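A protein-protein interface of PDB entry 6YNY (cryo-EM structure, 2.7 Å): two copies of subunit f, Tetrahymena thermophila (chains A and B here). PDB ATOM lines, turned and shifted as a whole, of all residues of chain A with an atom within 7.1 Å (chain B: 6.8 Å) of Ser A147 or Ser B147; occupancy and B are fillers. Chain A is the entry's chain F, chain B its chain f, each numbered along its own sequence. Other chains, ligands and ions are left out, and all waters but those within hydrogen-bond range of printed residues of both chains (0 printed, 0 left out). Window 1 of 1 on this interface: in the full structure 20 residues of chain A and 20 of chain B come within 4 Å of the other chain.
The backbone NH (N) of Gly A146 sits at hydrogen-bond distance from a ring nitrogen (ND1) of His B151 (3.0 Å). N of Phe A152 lies within hydrogen-bond range of O of Gly B146. The backbone NH (N) of Ser B147 sits at hydrogen-bond distance from the backbone carbonyl oxygen (O) of Ser A147 (3.3 Å). The backbone NH of Phe B152 lies within hydrogen-bond range of the backbone carbonyl oxygen of Gly A146 (2.8 Å). The backbone carbonyl oxygen (O) of Val A150 sits close to the backbone carbonyl oxygen (O) of Gly B146, at 3.2 Å. O of Gly A146 sits close to O of Val B150, at 3.3 Å. The side-chain hydroxyl (OG) of Ser A147 sits at hydrogen-bond distance from the backbone carbonyl oxygen (O) of Val B150. The backbone NH of Gly B146 is in hydrogen-bond range of a ring nitrogen (ND1) of His A151 (3.1 Å).
O of Gly A148 lies close to OE1 of Gln A134 (3.5 Å). A ring nitrogen (NE2) of His A151 sits close to the backbone carbonyl oxygen of Gln A149 (3.5 Å).
Among the printed residues, pairs that only touch across the chains: Val A150 with Ser B147 (3.5 Å), Glu A145 with Glu B145 (3.6 Å), Phe A152 with Gln B134 (3.6 Å), Ser A147 with Gly B146 (3.6 Å), Gln A134 with Phe B152 (3.6 Å), His A151 with Glu B145 (3.7 Å), Gly A148 with Gly B146 (3.7 Å), Phe A152 with Ile B144 (3.7 Å), Gly A146 with Ser B147 (3.8 Å), Glu A145 with His B151 (3.8 Å), Ile A144 with Phe B152 (3.8 Å) and Gly A146 with Gly B148 (3.9 Å).
Printed residues of chain B within 4 Å of Glu A145: Glu B145 and His B151. Of chain B, only Gly B146 (3.6 Å), Ser B147 (3.3 Å) and Val B150 (3.2 Å) come within 4 Å of Ser A147. Of the printed residues of chain B, Gly A148 touches Gly B146. Of the printed residues of chain B, Val A150 touches Gly B146 (3.2 Å) and Ser B147 (3.5 Å). Of the printed residues of chain A, Ile B144 touches Phe A152. Gln B149 touches none of the printed residues of chain A. Of the printed residues of chain A, His B151 touches Glu A145 and Gly A146. The nearest residue of chain A that does not touch Ser B147 is Phe A152 (4.5 Å).
Of the 11 printed residues of chain B, 9 touch a printed residue of chain A. Hydrophobic or aromatic side chains of chain B within 4 Å of the printed part of chain A: Ile B144, His B151 and Phe B152. Among the printed residues, 20 pairs touch across the chains. Among the printed residues, no Asp or Glu carboxylate lies within 4 Å of a Lys or Arg side-chain nitrogen of the other chain.
Gln A134 touches Phe B152, and with the chains exchanged Phe A152 touches Gln B134. Ile A144 touches Phe B152, and with the chains exchanged Phe A152 touches Ile B144. Gly A146 touches Phe B152, and with the chains exchanged Phe A152 touches Gly B146. Ser A147 touches its own counterpart, Ser B147. Of the 20 pairs that touch across the chains among the printed residues, 20 have their exchanged pair printed and touching as well.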
ATOM      1  N   TYR A 130      15.531  -6.182  31.706  1.00  0.00           N
ATOM      2  CA  TYR A 130      16.453  -5.800  30.645  1.00  0.00           C
ATOM      3  C   TYR A 130      15.708  -5.297  29.418  1.00  0.00           C
ATOM      4  O   TYR A 130      16.212  -4.425  28.704  1.00  0.00           O
ATOM      5  CB  TYR A 130      17.357  -6.973  30.272  1.00  0.00           C
ATOM      6  CG  TYR A 130      18.476  -6.596  29.334  1.00  0.00           C
ATOM      7  CD1 TYR A 130      19.669  -6.086  29.817  1.00  0.00           C
ATOM      8  CD2 TYR A 130      18.340  -6.745  27.966  1.00  0.00           C
ATOM      9  CE1 TYR A 130      20.688  -5.738  28.968  1.00  0.00           C
ATOM     10  CE2 TYR A 130      19.354  -6.401  27.110  1.00  0.00           C
ATOM     11  CZ  TYR A 130      20.525  -5.894  27.614  1.00  0.00           C
ATOM     12  OH  TYR A 130      21.543  -5.550  26.757  1.00  0.00           O
ATOM     13  N   GLN A 134      16.332  -1.801  27.379  1.00  0.00           N
ATOM     14  CA  GLN A 134      16.462  -1.620  25.942  1.00  0.00           C
ATOM     15  C   GLN A 134      15.431  -0.638  25.407  1.00  0.00           C
ATOM     16  O   GLN A 134      15.696   0.057  24.421  1.00  0.00           O
ATOM     17  CB  GLN A 134      16.342  -2.968  25.232  1.00  0.00           C
ATOM     18  CG  GLN A 134      17.596  -3.808  25.290  1.00  0.00           C
ATOM     19  CD  GLN A 134      17.550  -5.001  24.360  1.00  0.00           C
ATOM     20  OE1 GLN A 134      18.498  -5.262  23.621  1.00  0.00           O
ATOM     21  NE2 GLN A 134      16.449  -5.737  24.397  1.00  0.00           N
ATOM     22  N   ILE A 144      18.009  -0.379  17.875  1.00  0.00           N
ATOM     23  CA  ILE A 144      18.435  -1.694  18.326  1.00  0.00           C
ATOM     24  C   ILE A 144      18.095  -2.719  17.257  1.00  0.00           C
ATOM     25  O   ILE A 144      16.916  -2.961  16.974  1.00  0.00           O
ATOM     26  CB  ILE A 144      17.795  -2.069  19.666  1.00  0.00           C
ATOM     27  CG1 ILE A 144      18.343  -1.157  20.760  1.00  0.00           C
ATOM     28  CG2 ILE A 144      18.057  -3.517  19.986  1.00  0.00           C
ATOM     29  CD1 ILE A 144      17.568  -1.186  22.022  1.00  0.00           C
ATOM     30  N   GLU A 145      19.124  -3.317  16.665  1.00  0.00           N
ATOM     31  CA  GLU A 145      18.964  -4.482  15.812  1.00  0.00           C
ATOM     32  C   GLU A 145      19.043  -5.737  16.665  1.00  0.00           C
ATOM     33  O   GLU A 145      19.896  -5.851  17.550  1.00  0.00           O
ATOM     34  CB  GLU A 145      20.035  -4.526  14.724  1.00  0.00           C
ATOM     35  CG  GLU A 145      19.827  -3.549  13.591  1.00  0.00           C
ATOM     36  CD  GLU A 145      20.986  -3.529  12.619  1.00  0.00           C
ATOM     37  OE1 GLU A 145      22.096  -3.946  13.008  1.00  0.00           O
ATOM     38  OE2 GLU A 145      20.788  -3.099  11.464  1.00  0.00           O
ATOM     39  N   GLY A 146      18.151  -6.676  16.394  1.00  0.00           N
ATOM     40  CA  GLY A 146      18.077  -7.859  17.209  1.00  0.00           C
ATOM     41  C   GLY A 146      17.500  -7.530  18.573  1.00  0.00           C
ATOM     42  O   GLY A 146      16.788  -6.543  18.768  1.00  0.00           O
ATOM     43  N   SER A 147      17.829  -8.381  19.533  1.00  0.00           N
ATOM     44  CA  SER A 147      17.343  -8.221  20.894  1.00  0.00           C
ATOM     45  C   SER A 147      18.176  -9.114  21.797  1.00  0.00           C
ATOM     46  O   SER A 147      18.951  -9.953  21.333  1.00  0.00           O
ATOM     47  CB  SER A 147      15.858  -8.562  21.008  1.00  0.00           C
ATOM     48  OG  SER A 147      15.596  -9.848  20.480  1.00  0.00           O
ATOM     49  N   GLY A 148      18.004  -8.917  23.095  1.00  0.00           N
ATOM     50  CA  GLY A 148      18.725  -9.686  24.081  1.00  0.00           C
ATOM     51  C   GLY A 148      20.088  -9.111  24.387  1.00  0.00           C
ATOM     52  O   GLY A 148      20.525  -8.095  23.840  1.00  0.00           O
ATOM     53  N   GLN A 149      20.778  -9.796  25.294  1.00  0.00           N
ATOM     54  CA  GLN A 149      22.109  -9.405  25.729  1.00  0.00           C
ATOM     55  C   GLN A 149      23.149 -10.473  25.429  1.00  0.00           C
ATOM     56  O   GLN A 149      24.266 -10.403  25.953  1.00  0.00           O
ATOM     57  CB  GLN A 149      22.097  -9.086  27.225  1.00  0.00           C
ATOM     58  CG  GLN A 149      21.521 -10.187  28.078  1.00  0.00           C
ATOM     59  CD  GLN A 149      21.335  -9.771  29.518  1.00  0.00           C
ATOM     60  OE1 GLN A 149      22.237  -9.207  30.135  1.00  0.00           O
ATOM     61  NE2 GLN A 149      20.157 -10.035  30.058  1.00  0.00           N
ATOM     62  N   VAL A 150      22.813 -11.459  24.604  1.00  0.00           N
ATOM     63  CA  VAL A 150      23.783 -12.479  24.185  1.00  0.00           C
ATOM     64  C   VAL A 150      24.444 -11.932  22.927  1.00  0.00           C
ATOM     65  O   VAL A 150      24.076 -12.242  21.793  1.00  0.00           O
ATOM     66  CB  VAL A 150      23.130 -13.843  23.974  1.00  0.00           C
ATOM     67  CG1 VAL A 150      24.179 -14.884  23.717  1.00  0.00           C
ATOM     68  CG2 VAL A 150      22.296 -14.211  25.182  1.00  0.00           C
ATOM     69  N   HIS A 151      25.455 -11.100  23.136  1.00  0.00           N
ATOM     70  CA  HIS A 151      26.066 -10.357  22.044  1.00  0.00           C
ATOM     71  C   HIS A 151      26.830 -11.295  21.122  1.00  0.00           C
ATOM     72  O   HIS A 151      27.802 -11.936  21.532  1.00  0.00           O
ATOM     73  CB  HIS A 151      26.979  -9.274  22.605  1.00  0.00           C
ATOM     74  CG  HIS A 151      26.305  -8.387  23.600  1.00  0.00           C
ATOM     75  ND1 HIS A 151      25.197  -7.632  23.288  1.00  0.00           N
ATOM     76  CD2 HIS A 151      26.571  -8.143  24.903  1.00  0.00           C
ATOM     77  CE1 HIS A 151      24.811  -6.960  24.355  1.00  0.00           C
ATOM     78  NE2 HIS A 151      25.629  -7.250  25.348  1.00  0.00           N
ATOM     79  N   PHE A 152      26.379 -11.369  19.871  1.00  0.00           N
ATOM     80  CA  PHE A 152      27.039 -12.201  18.877  1.00  0.00           C
ATOM     81  C   PHE A 152      28.412 -11.659  18.513  1.00  0.00           C
ATOM     82  O   PHE A 152      29.295 -12.425  18.115  1.00  0.00           O
ATOM     83  CB  PHE A 152      26.154 -12.289  17.636  1.00  0.00           C
ATOM     84  CG  PHE A 152      26.691 -13.174  16.558  1.00  0.00           C
ATOM     85  CD1 PHE A 152      26.333 -14.503  16.495  1.00  0.00           C
ATOM     86  CD2 PHE A 152      27.539 -12.673  15.593  1.00  0.00           C
ATOM     87  CE1 PHE A 152      26.818 -15.312  15.504  1.00  0.00           C
ATOM     88  CE2 PHE A 152      28.026 -13.483  14.604  1.00  0.00           C
ATOM     89  CZ  PHE A 152      27.665 -14.804  14.558  1.00  0.00           C
ATOM     90  N   TYR B 130      21.011 -17.944   9.204  1.00  0.00           N
ATOM     91  CA  TYR B 130      21.054 -16.529   9.550  1.00  0.00           C
ATOM     92  C   TYR B 130      22.232 -16.216  10.462  1.00  0.00           C
ATOM     93  O   TYR B 130      22.721 -15.082  10.471  1.00  0.00           O
ATOM     94  CB  TYR B 130      19.742 -16.099  10.206  1.00  0.00           C
ATOM     95  CG  TYR B 130      19.665 -14.618  10.466  1.00  0.00           C
ATOM     96  CD1 TYR B 130      19.214 -13.747   9.492  1.00  0.00           C
ATOM     97  CD2 TYR B 130      20.052 -14.093  11.682  1.00  0.00           C
ATOM     98  CE1 TYR B 130      19.150 -12.396   9.725  1.00  0.00           C
ATOM     99  CE2 TYR B 130      19.992 -12.746  11.923  1.00  0.00           C
ATOM    100  CZ  TYR B 130      19.543 -11.898  10.940  1.00  0.00           C
ATOM    101  OH  TYR B 130      19.475 -10.547  11.173  1.00  0.00           O
ATOM    102  N   GLN B 134      25.160 -13.411  10.044  1.00  0.00           N
ATOM    103  CA  GLN B 134      25.641 -12.470  11.046  1.00  0.00           C
ATOM    104  C   GLN B 134      27.144 -12.580  11.238  1.00  0.00           C
ATOM    105  O   GLN B 134      27.803 -11.585  11.556  1.00  0.00           O
ATOM    106  CB  GLN B 134      24.922 -12.694  12.375  1.00  0.00           C
ATOM    107  CG  GLN B 134      23.516 -12.132  12.436  1.00  0.00           C
ATOM    108  CD  GLN B 134      22.999 -12.024  13.854  1.00  0.00           C
ATOM    109  OE1 GLN B 134      22.417 -11.012  14.240  1.00  0.00           O
ATOM    110  NE2 GLN B 134      23.206 -13.072  14.638  1.00  0.00           N
ATOM    111  N   ILE B 144      28.068  -6.558  16.246  1.00  0.00           N
ATOM    112  CA  ILE B 144      26.692  -6.974  16.473  1.00  0.00           C
ATOM    113  C   ILE B 144      26.444  -7.077  17.968  1.00  0.00           C
ATOM    114  O   ILE B 144      27.046  -7.917  18.648  1.00  0.00           O
ATOM    115  CB  ILE B 144      26.379  -8.303  15.776  1.00  0.00           C
ATOM    116  CG1 ILE B 144      26.504  -8.126  14.266  1.00  0.00           C
ATOM    117  CG2 ILE B 144      24.996  -8.782  16.158  1.00  0.00           C
ATOM    118  CD1 ILE B 144      26.454  -9.387  13.492  1.00  0.00           C
ATOM    119  N   GLU B 145      25.565  -6.223  18.481  1.00  0.00           N
ATOM    120  CA  GLU B 145      25.005  -6.386  19.810  1.00  0.00           C
ATOM    121  C   GLU B 145      23.738  -7.222  19.719  1.00  0.00           C
ATOM    122  O   GLU B 145      22.992  -7.149  18.738  1.00  0.00           O
ATOM    123  CB  GLU B 145      24.695  -5.036  20.453  1.00  0.00           C
ATOM    124  CG  GLU B 145      25.907  -4.261  20.893  1.00  0.00           C
ATOM    125  CD  GLU B 145      25.557  -2.903  21.461  1.00  0.00           C
ATOM    126  OE1 GLU B 145      24.364  -2.660  21.733  1.00  0.00           O
ATOM    127  OE2 GLU B 145      26.473  -2.072  21.629  1.00  0.00           O
ATOM    128  N   GLY B 146      23.504  -8.023  20.747  1.00  0.00           N
ATOM    129  CA  GLY B 146      22.372  -8.912  20.722  1.00  0.00           C
ATOM    130  C   GLY B 146      22.565 -10.018  19.701  1.00  0.00           C
ATOM    131  O   GLY B 146      23.674 -10.324  19.260  1.00  0.00           O
ATOM    132  N   SER B 147      21.444 -10.614  19.315  1.00  0.00           N
ATOM    133  CA  SER B 147      21.458 -11.723  18.374  1.00  0.00           C
ATOM    134  C   SER B 147      20.058 -11.904  17.812  1.00  0.00           C
ATOM    135  O   SER B 147      19.087 -11.325  18.302  1.00  0.00           O
ATOM    136  CB  SER B 147      21.948 -13.007  19.043  1.00  0.00           C
ATOM    137  OG  SER B 147      21.160 -13.310  20.177  1.00  0.00           O
ATOM    138  N   GLY B 148      19.972 -12.714  16.765  1.00  0.00           N
ATOM    139  CA  GLY B 148      18.705 -13.010  16.137  1.00  0.00           C
ATOM    140  C   GLY B 148      18.262 -11.916  15.188  1.00  0.00           C
ATOM    141  O   GLY B 148      18.956 -10.930  14.938  1.00  0.00           O
ATOM    142  N   GLN B 149      17.061 -12.108  14.647  1.00  0.00           N
ATOM    143  CA  GLN B 149      16.457 -11.161  13.720  1.00  0.00           C
ATOM    144  C   GLN B 149      15.145 -10.591  14.240  1.00  0.00           C
ATOM    145  O   GLN B 149      14.395  -9.985  13.468  1.00  0.00           O
ATOM    146  CB  GLN B 149      16.235 -11.822  12.360  1.00  0.00           C
ATOM    147  CG  GLN B 149      15.737 -13.243  12.434  1.00  0.00           C
ATOM    148  CD  GLN B 149      15.559 -13.863  11.073  1.00  0.00           C
ATOM    149  OE1 GLN B 149      15.099 -13.214  10.136  1.00  0.00           O
ATOM    150  NE2 GLN B 149      15.932 -15.126  10.952  1.00  0.00           N
ATOM    151  N   VAL B 150      14.848 -10.771  15.522  1.00  0.00           N
ATOM    152  CA  VAL B 150      13.646 -10.178  16.124  1.00  0.00           C
ATOM    153  C   VAL B 150      14.065  -8.796  16.606  1.00  0.00           C
ATOM    154  O   VAL B 150      14.380  -8.565  17.775  1.00  0.00           O
ATOM    155  CB  VAL B 150      13.069 -11.054  17.235  1.00  0.00           C
ATOM    156  CG1 VAL B 150      11.807 -10.449  17.785  1.00  0.00           C
ATOM    157  CG2 VAL B 150      12.795 -12.433  16.702  1.00  0.00           C
ATOM    158  N   HIS B 151      14.049  -7.847  15.678  1.00  0.00           N
ATOM    159  CA  HIS B 151      14.576  -6.517  15.940  1.00  0.00           C
ATOM    160  C   HIS B 151      13.699  -5.793  16.951  1.00  0.00           C
ATOM    161  O   HIS B 151      12.523  -5.524  16.690  1.00  0.00           O
ATOM    162  CB  HIS B 151      14.668  -5.732  14.639  1.00  0.00           C
ATOM    163  CG  HIS B 151      15.436  -6.438  13.566  1.00  0.00           C
ATOM    164  ND1 HIS B 151      16.774  -6.738  13.685  1.00  0.00           N
ATOM    165  CD2 HIS B 151      15.054  -6.900  12.354  1.00  0.00           C
ATOM    166  CE1 HIS B 151      17.183  -7.359  12.594  1.00  0.00           C
ATOM    167  NE2 HIS B 151      16.159  -7.469  11.770  1.00  0.00           N
ATOM    168  N   PHE B 152      14.283  -5.479  18.106  1.00  0.00           N
ATOM    169  CA  PHE B 152      13.553  -4.791  19.161  1.00  0.00           C
ATOM    170  C   PHE B 152      13.203  -3.364  18.774  1.00  0.00           C
ATOM    171  O   PHE B 152      12.194  -2.828  19.242  1.00  0.00           O
ATOM    172  CB  PHE B 152      14.387  -4.798  20.441  1.00  0.00           C
ATOM    173  CG  PHE B 152      13.718  -4.157  21.615  1.00  0.00           C
ATOM    174  CD1 PHE B 152      12.940  -4.902  22.477  1.00  0.00           C
ATOM    175  CD2 PHE B 152      13.884  -2.813  21.870  1.00  0.00           C
ATOM    176  CE1 PHE B 152      12.334  -4.314  23.558  1.00  0.00           C
ATOM    177  CE2 PHE B 152      13.278  -2.224  22.946  1.00  0.00           C
ATOM    178  CZ  PHE B 152      12.504  -2.973  23.793  1.00  0.00           C
